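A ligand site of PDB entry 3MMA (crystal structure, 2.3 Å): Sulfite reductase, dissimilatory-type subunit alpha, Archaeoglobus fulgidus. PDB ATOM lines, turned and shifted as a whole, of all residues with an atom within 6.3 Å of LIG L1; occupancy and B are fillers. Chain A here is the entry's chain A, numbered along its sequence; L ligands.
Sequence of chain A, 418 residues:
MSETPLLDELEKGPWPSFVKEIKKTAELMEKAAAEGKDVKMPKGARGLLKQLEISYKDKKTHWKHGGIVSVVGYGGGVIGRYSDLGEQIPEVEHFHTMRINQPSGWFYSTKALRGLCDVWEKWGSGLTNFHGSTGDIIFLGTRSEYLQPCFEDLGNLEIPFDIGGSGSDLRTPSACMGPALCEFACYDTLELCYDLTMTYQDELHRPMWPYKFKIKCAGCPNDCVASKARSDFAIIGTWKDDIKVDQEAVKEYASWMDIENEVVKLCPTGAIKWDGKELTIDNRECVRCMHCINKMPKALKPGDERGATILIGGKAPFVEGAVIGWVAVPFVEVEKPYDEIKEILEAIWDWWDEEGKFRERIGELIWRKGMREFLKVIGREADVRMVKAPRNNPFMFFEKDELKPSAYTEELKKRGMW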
ATOM      1  N   CYS A 176     -17.268  19.209  -2.792  1.00  0.00           N
ATOM      2  CA  CYS A 176     -16.130  18.293  -2.891  1.00  0.00           C
ATOM      3  C   CYS A 176     -15.842  18.115  -4.374  1.00  0.00           C
ATOM      4  O   CYS A 176     -16.708  18.389  -5.207  1.00  0.00           O
ATOM      5  CB  CYS A 176     -16.482  16.906  -2.299  1.00  0.00           C
ATOM      6  SG  CYS A 176     -17.592  16.091  -3.424  1.00  0.00           S
ATOM      7  N   MET A 177     -14.668  17.591  -4.701  1.00  0.00           N
ATOM      8  CA  MET A 177     -14.282  17.323  -6.109  1.00  0.00           C
ATOM      9  C   MET A 177     -15.337  16.631  -6.956  1.00  0.00           C
ATOM     10  O   MET A 177     -15.432  16.877  -8.165  1.00  0.00           O
ATOM     11  CB  MET A 177     -12.963  16.538  -6.186  1.00  0.00           C
ATOM     12  CG  MET A 177     -13.028  15.064  -5.724  1.00  0.00           C
ATOM     13  SD  MET A 177     -11.369  14.444  -5.405  1.00  0.00           S
ATOM     14  CE  MET A 177     -11.630  12.648  -5.277  1.00  0.00           C
ATOM     15  N   GLY A 178     -16.124  15.748  -6.352  1.00  0.00           N
ATOM     16  CA  GLY A 178     -17.180  15.049  -7.072  1.00  0.00           C
ATOM     17  C   GLY A 178     -16.748  14.362  -8.369  1.00  0.00           C
ATOM     18  O   GLY A 178     -15.637  13.862  -8.472  1.00  0.00           O
ATOM     19  N   PRO A 179     -17.643  14.367  -9.389  1.00  0.00           N
ATOM     20  CA  PRO A 179     -17.463  13.553 -10.596  1.00  0.00           C
ATOM     21  C   PRO A 179     -16.244  13.987 -11.430  1.00  0.00           C
ATOM     22  O   PRO A 179     -15.836  13.265 -12.362  1.00  0.00           O
ATOM     23  CB  PRO A 179     -18.785  13.772 -11.365  1.00  0.00           C
ATOM     24  CG  PRO A 179     -19.239  15.160 -10.922  1.00  0.00           C
ATOM     25  CD  PRO A 179     -18.841  15.241  -9.462  1.00  0.00           C
ATOM     26  N   CYS A 182     -13.866  11.715  -8.924  1.00  0.00           N
ATOM     27  CA  CYS A 182     -14.285  10.669  -7.973  1.00  0.00           C
ATOM     28  C   CYS A 182     -15.300   9.684  -8.554  1.00  0.00           C
ATOM     29  O   CYS A 182     -16.345  10.094  -9.071  1.00  0.00           O
ATOM     30  CB  CYS A 182     -14.848  11.324  -6.722  1.00  0.00           C
ATOM     31  SG  CYS A 182     -14.978  10.206  -5.302  1.00  0.00           S
ATOM     32  N   GLU A 183     -15.009   8.386  -8.444  1.00  0.00           N
ATOM     33  CA  GLU A 183     -15.919   7.357  -8.956  1.00  0.00           C
ATOM     34  C   GLU A 183     -17.090   7.085  -8.007  1.00  0.00           C
ATOM     35  O   GLU A 183     -17.995   6.295  -8.321  1.00  0.00           O
ATOM     36  CB  GLU A 183     -15.145   6.080  -9.274  1.00  0.00           C
ATOM     37  CG  GLU A 183     -14.735   5.246  -8.053  1.00  0.00           C
ATOM     38  CD  GLU A 183     -13.378   5.595  -7.504  1.00  0.00           C
ATOM     39  OE1 GLU A 183     -12.980   6.806  -7.566  1.00  0.00           O
ATOM     40  OE2 GLU A 183     -12.720   4.670  -6.987  1.00  0.00           O
ATOM     41  N   PHE A 184     -17.082   7.757  -6.858  1.00  0.00           N
ATOM     42  CA  PHE A 184     -18.143   7.609  -5.837  1.00  0.00           C
ATOM     43  C   PHE A 184     -19.288   8.620  -5.967  1.00  0.00           C
ATOM     44  O   PHE A 184     -20.339   8.451  -5.347  1.00  0.00           O
ATOM     45  CB  PHE A 184     -17.575   7.715  -4.416  1.00  0.00           C
ATOM     46  CG  PHE A 184     -16.561   6.652  -4.056  1.00  0.00           C
ATOM     47  CD1 PHE A 184     -16.419   5.491  -4.805  1.00  0.00           C
ATOM     48  CD2 PHE A 184     -15.730   6.825  -2.939  1.00  0.00           C
ATOM     49  CE1 PHE A 184     -15.482   4.536  -4.461  1.00  0.00           C
ATOM     50  CE2 PHE A 184     -14.786   5.867  -2.588  1.00  0.00           C
ATOM     51  CZ  PHE A 184     -14.668   4.720  -3.351  1.00  0.00           C
ATOM     52  N   ALA A 185     -19.108   9.655  -6.771  1.00  0.00           N
ATOM     53  CA  ALA A 185     -20.075  10.762  -6.831  1.00  0.00           C
ATOM     54  C   ALA A 185     -21.476  10.266  -7.154  1.00  0.00           C
ATOM     55  O   ALA A 185     -21.648   9.453  -8.061  1.00  0.00           O
ATOM     56  CB  ALA A 185     -19.630  11.779  -7.845  1.00  0.00           C
ATOM     57  N   CYS A 186     -22.471  10.734  -6.406  1.00  0.00           N
ATOM     58  CA  CYS A 186     -23.859  10.442  -6.723  1.00  0.00           C
ATOM     59  C   CYS A 186     -24.589  11.560  -7.482  1.00  0.00           C
ATOM     60  O   CYS A 186     -25.654  11.312  -8.070  1.00  0.00           O
ATOM     61  CB  CYS A 186     -24.602  10.026  -5.461  1.00  0.00           C
ATOM     62  SG  CYS A 186     -23.886   8.524  -4.803  1.00  0.00           S
ATOM     63  N   THR A 189     -21.511  17.616  -7.988  1.00  0.00           N
ATOM     64  CA  THR A 189     -21.353  18.595  -6.906  1.00  0.00           C
ATOM     65  C   THR A 189     -20.921  19.974  -7.420  1.00  0.00           C
ATOM     66  O   THR A 189     -21.490  21.010  -7.028  1.00  0.00           O
ATOM     67  CB  THR A 189     -20.367  18.096  -5.814  1.00  0.00           C
ATOM     68  OG1 THR A 189     -19.079  17.868  -6.392  1.00  0.00           O
ATOM     69  CG2 THR A 189     -20.872  16.792  -5.177  1.00  0.00           C
ATOM     70  N   CYS A 217     -21.952  20.948  -0.540  1.00  0.00           N
ATOM     71  CA  CYS A 217     -22.372  19.884  -1.437  1.00  0.00           C
ATOM     72  C   CYS A 217     -21.380  18.760  -1.405  1.00  0.00           C
ATOM     73  O   CYS A 217     -20.250  18.926  -1.859  1.00  0.00           O
ATOM     74  CB  CYS A 217     -22.460  20.414  -2.872  1.00  0.00           C
ATOM     75  SG  CYS A 217     -23.563  21.778  -3.065  1.00  0.00           S
ATOM     76  N   ALA A 218     -21.798  17.619  -0.901  1.00  0.00           N
ATOM     77  CA  ALA A 218     -20.941  16.450  -0.846  1.00  0.00           C
ATOM     78  C   ALA A 218     -21.522  15.372  -1.769  1.00  0.00           C
ATOM     79  O   ALA A 218     -22.725  15.097  -1.741  1.00  0.00           O
ATOM     80  CB  ALA A 218     -20.843  15.942   0.560  1.00  0.00           C
ATOM     81  N   GLY A 219     -20.647  14.767  -2.569  1.00  0.00           N
ATOM     82  CA  GLY A 219     -21.107  13.872  -3.635  1.00  0.00           C
ATOM     83  C   GLY A 219     -21.603  12.536  -3.145  1.00  0.00           C
ATOM     84  O   GLY A 219     -22.282  11.817  -3.869  1.00  0.00           O
ATOM     85  N   CYS A 220     -21.277  12.198  -1.902  1.00  0.00           N
ATOM     86  CA  CYS A 220     -21.642  10.859  -1.393  1.00  0.00           C
ATOM     87  C   CYS A 220     -21.491  10.913   0.116  1.00  0.00           C
ATOM     88  O   CYS A 220     -20.968  11.905   0.634  1.00  0.00           O
ATOM     89  CB  CYS A 220     -20.747   9.789  -2.045  1.00  0.00           C
ATOM     90  SG  CYS A 220     -19.227   9.437  -1.213  1.00  0.00           S
ATOM     91  N   PRO A 221     -21.986   9.872   0.842  1.00  0.00           N
ATOM     92  CA  PRO A 221     -22.003   9.915   2.319  1.00  0.00           C
ATOM     93  C   PRO A 221     -20.658  10.093   3.030  1.00  0.00           C
ATOM     94  O   PRO A 221     -20.649  10.374   4.232  1.00  0.00           O
ATOM     95  CB  PRO A 221     -22.659   8.583   2.691  1.00  0.00           C
ATOM     96  CG  PRO A 221     -23.595   8.306   1.534  1.00  0.00           C
ATOM     97  CD  PRO A 221     -22.769   8.728   0.325  1.00  0.00           C
ATOM     98  N   ASN A 222     -19.546   9.976   2.303  1.00  0.00           N
ATOM     99  CA  ASN A 222     -18.219  10.195   2.904  1.00  0.00           C
ATOM    100  C   ASN A 222     -18.037  11.633   3.368  1.00  0.00           C
ATOM    101  O   ASN A 222     -17.220  11.899   4.237  1.00  0.00           O
ATOM    102  CB  ASN A 222     -17.069   9.743   1.990  1.00  0.00           C
ATOM    103  CG  ASN A 222     -16.865   8.186   2.000  1.00  0.00           C
ATOM    104  OD1 ASN A 222     -17.016   7.540   3.034  1.00  0.00           O
ATOM    105  ND2 ASN A 222     -16.481   7.630   0.853  1.00  0.00           N
ATOM    106  N   ASP A 223     -18.820  12.542   2.793  1.00  0.00           N
ATOM    107  CA  ASP A 223     -18.883  13.945   3.176  1.00  0.00           C
ATOM    108  C   ASP A 223     -17.520  14.635   3.295  1.00  0.00           C
ATOM    109  O   ASP A 223     -17.147  15.183   4.341  1.00  0.00           O
ATOM    110  CB  ASP A 223     -19.716  14.123   4.458  1.00  0.00           C
ATOM    111  CG  ASP A 223     -20.194  15.555   4.644  1.00  0.00           C
ATOM    112  OD1 ASP A 223     -20.761  15.880   5.704  1.00  0.00           O
ATOM    113  OD2 ASP A 223     -20.009  16.345   3.716  1.00  0.00           O
ATOM    114  N   CYS A 224     -16.795  14.629   2.177  1.00  0.00           N
ATOM    115  CA  CYS A 224     -15.427  15.162   2.091  1.00  0.00           C
ATOM    116  C   CYS A 224     -15.336  16.711   2.114  1.00  0.00           C
ATOM    117  O   CYS A 224     -14.249  17.269   1.960  1.00  0.00           O
ATOM    118  CB  CYS A 224     -14.714  14.507   0.871  1.00  0.00           C
ATOM    119  SG  CYS A 224     -14.640  12.560   0.871  1.00  0.00           S
ATOM    120  N   VAL A 225     -16.461  17.416   2.279  1.00  0.00           N
ATOM    121  CA  VAL A 225     -16.451  18.862   2.538  1.00  0.00           C
ATOM    122  C   VAL A 225     -16.970  19.220   3.906  1.00  0.00           C
ATOM    123  O   VAL A 225     -17.215  20.406   4.208  1.00  0.00           O
ATOM    124  CB  VAL A 225     -17.250  19.734   1.496  1.00  0.00           C
ATOM    125  CG1 VAL A 225     -16.348  20.145   0.382  1.00  0.00           C
ATOM    126  CG2 VAL A 225     -18.545  19.066   1.038  1.00  0.00           C
ATOM    127  N   MET A 290     -20.951   3.434   3.122  1.00  0.00           N
ATOM    128  CA  MET A 290     -19.862   3.537   2.116  1.00  0.00           C
ATOM    129  C   MET A 290     -18.590   2.733   2.360  1.00  0.00           C
ATOM    130  O   MET A 290     -17.835   2.475   1.418  1.00  0.00           O
ATOM    131  CB  MET A 290     -19.490   5.002   1.818  1.00  0.00           C
ATOM    132  CG  MET A 290     -20.601   5.758   1.166  1.00  0.00           C
ATOM    133  SD  MET A 290     -20.765   5.200  -0.518  1.00  0.00           S
ATOM    134  CE  MET A 290     -19.266   5.948  -1.228  1.00  0.00           C
ATOM    135  N   ASN A 294     -15.797   1.864  -0.129  1.00  0.00           N
ATOM    136  CA  ASN A 294     -14.439   2.375   0.211  1.00  0.00           C
ATOM    137  C   ASN A 294     -13.376   1.274   0.242  1.00  0.00           C
ATOM    138  O   ASN A 294     -12.272   1.474  -0.246  1.00  0.00           O
ATOM    139  CB  ASN A 294     -14.420   3.152   1.531  1.00  0.00           C
ATOM    140  CG  ASN A 294     -15.401   4.316   1.561  1.00  0.00           C
ATOM    141  OD1 ASN A 294     -15.881   4.767   0.519  1.00  0.00           O
ATOM    142  ND2 ASN A 294     -15.751   4.758   2.760  1.00  0.00           N
HETATM  143 FE1  LIG L   1     -17.951  11.255  -1.897  1.00  0.00          FE
HETATM  144 FE2  LIG L   1     -15.690  12.455  -1.122  1.00  0.00          FE
HETATM  145 FE3  LIG L   1     -15.943  11.303  -3.625  1.00  0.00          FE
HETATM  146 FE4  LIG L   1     -17.129  13.649  -2.850  1.00  0.00          FE
HETATM  147  S1  LIG L   1     -14.894  13.235  -3.091  1.00  0.00           S
HETATM  148  S2  LIG L   1     -18.092  11.883  -4.055  1.00  0.00           S
HETATM  149  S3  LIG L   1     -17.814  13.245  -0.732  1.00  0.00           S
HETATM  150  S4  LIG L   1     -15.924  10.217  -1.609  1.00  0.00           S
HETATM  151 FE1  LG2 L   2     -12.380  12.049   1.407  1.00  0.00          FE
HETATM  152  C1  LG2 L   2     -12.317   8.727   0.608  1.00  0.00           C
HETATM  153  C2  LG2 L   2     -10.969  12.716  -1.446  1.00  0.00           C
HETATM  154  C3  LG2 L   2     -11.554  15.107   2.526  1.00  0.00           C
HETATM  155  C4  LG2 L   2     -13.608  11.301   4.357  1.00  0.00           C
HETATM  156  N1  LG2 L   2     -11.799  10.995  -0.108  1.00  0.00           N
HETATM  157  C5  LG2 L   2     -11.937   9.676  -0.328  1.00  0.00           C
HETATM  158  C6  LG2 L   2     -11.590   9.198  -1.709  1.00  0.00           C
HETATM  159  C7  LG2 L   2     -10.756   7.897  -1.595  1.00  0.00           C
HETATM  160  C8  LG2 L   2     -12.674   8.899  -2.736  1.00  0.00           C
HETATM  161  C9  LG2 L   2     -12.212   8.475  -4.118  1.00  0.00           C
HETATM  162  O1  LG2 L   2     -11.276   9.076  -4.739  1.00  0.00           O
HETATM  163  O2  LG2 L   2     -12.873   7.529  -4.590  1.00  0.00           O
HETATM  164  C10 LG2 L   2     -10.837  10.391  -2.222  1.00  0.00           C
HETATM  165  C11 LG2 L   2      -9.307  10.137  -2.085  1.00  0.00           C
HETATM  166  C12 LG2 L   2      -8.722  10.322  -0.664  1.00  0.00           C
HETATM  167  C13 LG2 L   2      -7.496   9.539  -0.242  1.00  0.00           C
HETATM  168  O3  LG2 L   2      -6.426  10.136   0.045  1.00  0.00           O
HETATM  169  O4  LG2 L   2      -7.566   8.280  -0.149  1.00  0.00           O
HETATM  170  C14 LG2 L   2     -11.211  11.407  -1.169  1.00  0.00           C
HETATM  171  N2  LG2 L   2     -11.482  13.579   0.642  1.00  0.00           N
HETATM  172  C15 LG2 L   2     -11.035  13.716  -0.574  1.00  0.00           C
HETATM  173  C16 LG2 L   2     -10.573  15.091  -1.031  1.00  0.00           C
HETATM  174  C17 LG2 L   2      -9.439  15.124  -2.063  1.00  0.00           C
HETATM  175  C18 LG2 L   2     -11.831  15.839  -1.550  1.00  0.00           C
HETATM  176  C19 LG2 L   2     -11.808  17.291  -2.052  1.00  0.00           C
HETATM  177  O5  LG2 L   2     -12.727  17.674  -2.809  1.00  0.00           O
HETATM  178  O6  LG2 L   2     -10.921  18.095  -1.702  1.00  0.00           O
HETATM  179  C20 LG2 L   2     -10.453  15.609   0.338  1.00  0.00           C
HETATM  180  C21 LG2 L   2      -9.230  16.436   0.752  1.00  0.00           C
HETATM  181  C22 LG2 L   2      -8.552  16.086   2.102  1.00  0.00           C
HETATM  182  C23 LG2 L   2      -7.040  16.233   2.319  1.00  0.00           C
HETATM  183  O7  LG2 L   2      -6.283  17.041   1.701  1.00  0.00           O
HETATM  184  O8  LG2 L   2      -6.545  15.501   3.200  1.00  0.00           O
HETATM  185  C24 LG2 L   2     -11.230  14.757   1.271  1.00  0.00           C
HETATM  186  N3  LG2 L   2     -12.648  13.031   3.071  1.00  0.00           N
HETATM  187  C25 LG2 L   2     -12.262  14.268   3.313  1.00  0.00           C
HETATM  188  C26 LG2 L   2     -12.604  14.731   4.697  1.00  0.00           C
HETATM  189  C27 LG2 L   2     -13.292  16.080   4.962  1.00  0.00           C
HETATM  190  C28 LG2 L   2     -12.404  16.709   6.040  1.00  0.00           C
HETATM  191  O9  LG2 L   2     -11.530  15.987   6.600  1.00  0.00           O
HETATM  192  O10 LG2 L   2     -12.549  17.932   6.332  1.00  0.00           O
HETATM  193  C29 LG2 L   2     -13.158  13.478   5.329  1.00  0.00           C
HETATM  194  C30 LG2 L   2     -14.346  13.614   6.275  1.00  0.00           C
HETATM  195  C31 LG2 L   2     -13.643  13.543   7.647  1.00  0.00           C
HETATM  196  C32 LG2 L   2     -14.309  12.595   8.625  1.00  0.00           C
HETATM  197  O11 LG2 L   2     -14.380  12.922   9.819  1.00  0.00           O
HETATM  198  O12 LG2 L   2     -14.771  11.505   8.225  1.00  0.00           O
HETATM  199  C33 LG2 L   2     -13.173  12.563   4.152  1.00  0.00           C
HETATM  200  N4  LG2 L   2     -12.954  10.402   2.294  1.00  0.00           N
HETATM  201  C34 LG2 L   2     -13.469  10.269   3.519  1.00  0.00           C
HETATM  202  C35 LG2 L   2     -13.982   8.882   3.906  1.00  0.00           C
HETATM  203  C36 LG2 L   2     -13.990   8.295   5.339  1.00  0.00           C
HETATM  204  C37 LG2 L   2     -12.813   7.578   5.987  1.00  0.00           C
HETATM  205  C38 LG2 L   2     -13.297   6.800   7.212  1.00  0.00           C
HETATM  206  O13 LG2 L   2     -12.756   5.707   7.448  1.00  0.00           O
HETATM  207  O14 LG2 L   2     -14.210   7.249   7.975  1.00  0.00           O
HETATM  208  C39 LG2 L   2     -13.521   8.085   2.698  1.00  0.00           C
HETATM  209  C40 LG2 L   2     -13.092   6.617   2.786  1.00  0.00           C
HETATM  210  C41 LG2 L   2     -11.690   6.181   2.464  1.00  0.00           C
HETATM  211  O15 LG2 L   2     -10.834   6.223   3.382  1.00  0.00           O
HETATM  212  O16 LG2 L   2     -11.469   5.748   1.303  1.00  0.00           O
HETATM  213  C42 LG2 L   2     -12.860   9.125   1.816  1.00  0.00           C
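The side-chain sulfur of Cys 182 sits close to the backbone NH of Phe 184 (3.6 Å).
The side-chain sulfur (SG) of Cys 220 lies close to the backbone NH (N) of Asn 222 (3.6 Å).
SG of Cys 176 lies close to N of Gly 219.
N of Gly 178 sits close to SG of Cys 176 (3.3 Å).
O of Cys 176 is in hydrogen-bond range of OG1 of Thr 189 (2.7 Å).
The backbone NH of Cys 176 is in hydrogen-bond range of the backbone carbonyl oxygen of Cys 217, at 3.1 Å.
ND2 of Asn 222 sits at hydrogen-bond distance from OD1 of Asn 294 (2.9 Å).
The backbone NH of Cys 186 lies within hydrogen-bond range of the backbone carbonyl oxygen of Gly 219, at 2.8 Å.
FE3 of LIG L1 is bound by SG of Cys 182 (2.2 Å).
A sulfur (S3) of LIG L1 lies close to the backbone NH (N) of Cys 224 (3.4 Å).
The side-chain sulfur (SG) of Cys 224 is bound to an iron atom (FE2) of LIG L1 (2.3 Å).
FE1 of LIG L1 is bound by SG of Cys 220 (2.3 Å).
The side-chain sulfur (SG) of Cys 176 is bound to an iron atom (FE4) of LIG L1.
The backbone NH of Ala 185 sits close to a sulfur (S2) of LIG L1 (3.7 Å).
A sulfur (S4) of LIG L1 sits close to the side-chain amide nitrogen (ND2) of Asn 222 (3.6 Å).
The backbone NH of Gly 219 sits close to a sulfur (S3) of LIG L1 (3.7 Å).
A sulfur (S3) of LIG L1 lies close to the backbone NH (N) of Asp 223.
O2 of LG2 L2 sits close to SG of Cys 182 (3.5 Å).
SG of Cys 224 binds FE1 of LG2 L2, 2.4 Å away.
The backbone NH (N) of Met 177 lies within hydrogen-bond range of an oxygen (O5) of LG2 L2, 2.7 Å away.
An oxygen (O2) of LG2 L2 sits close to the side-chain carboxylate of Glu 183, at 3.1 Å.
Residues that only touch LIG L1: Phe 184 and Met 177.
Ten residues have an atom within 4 Å of LIG L1: Cys 176, Met 177, Cys 182, Phe 184, Ala 185, Gly 219, Cys 220, Asn 222, Asp 223 and Cys 224.
The nearest printed residue that does not touch LIG L1 is Gly 178 (4.2 Å).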
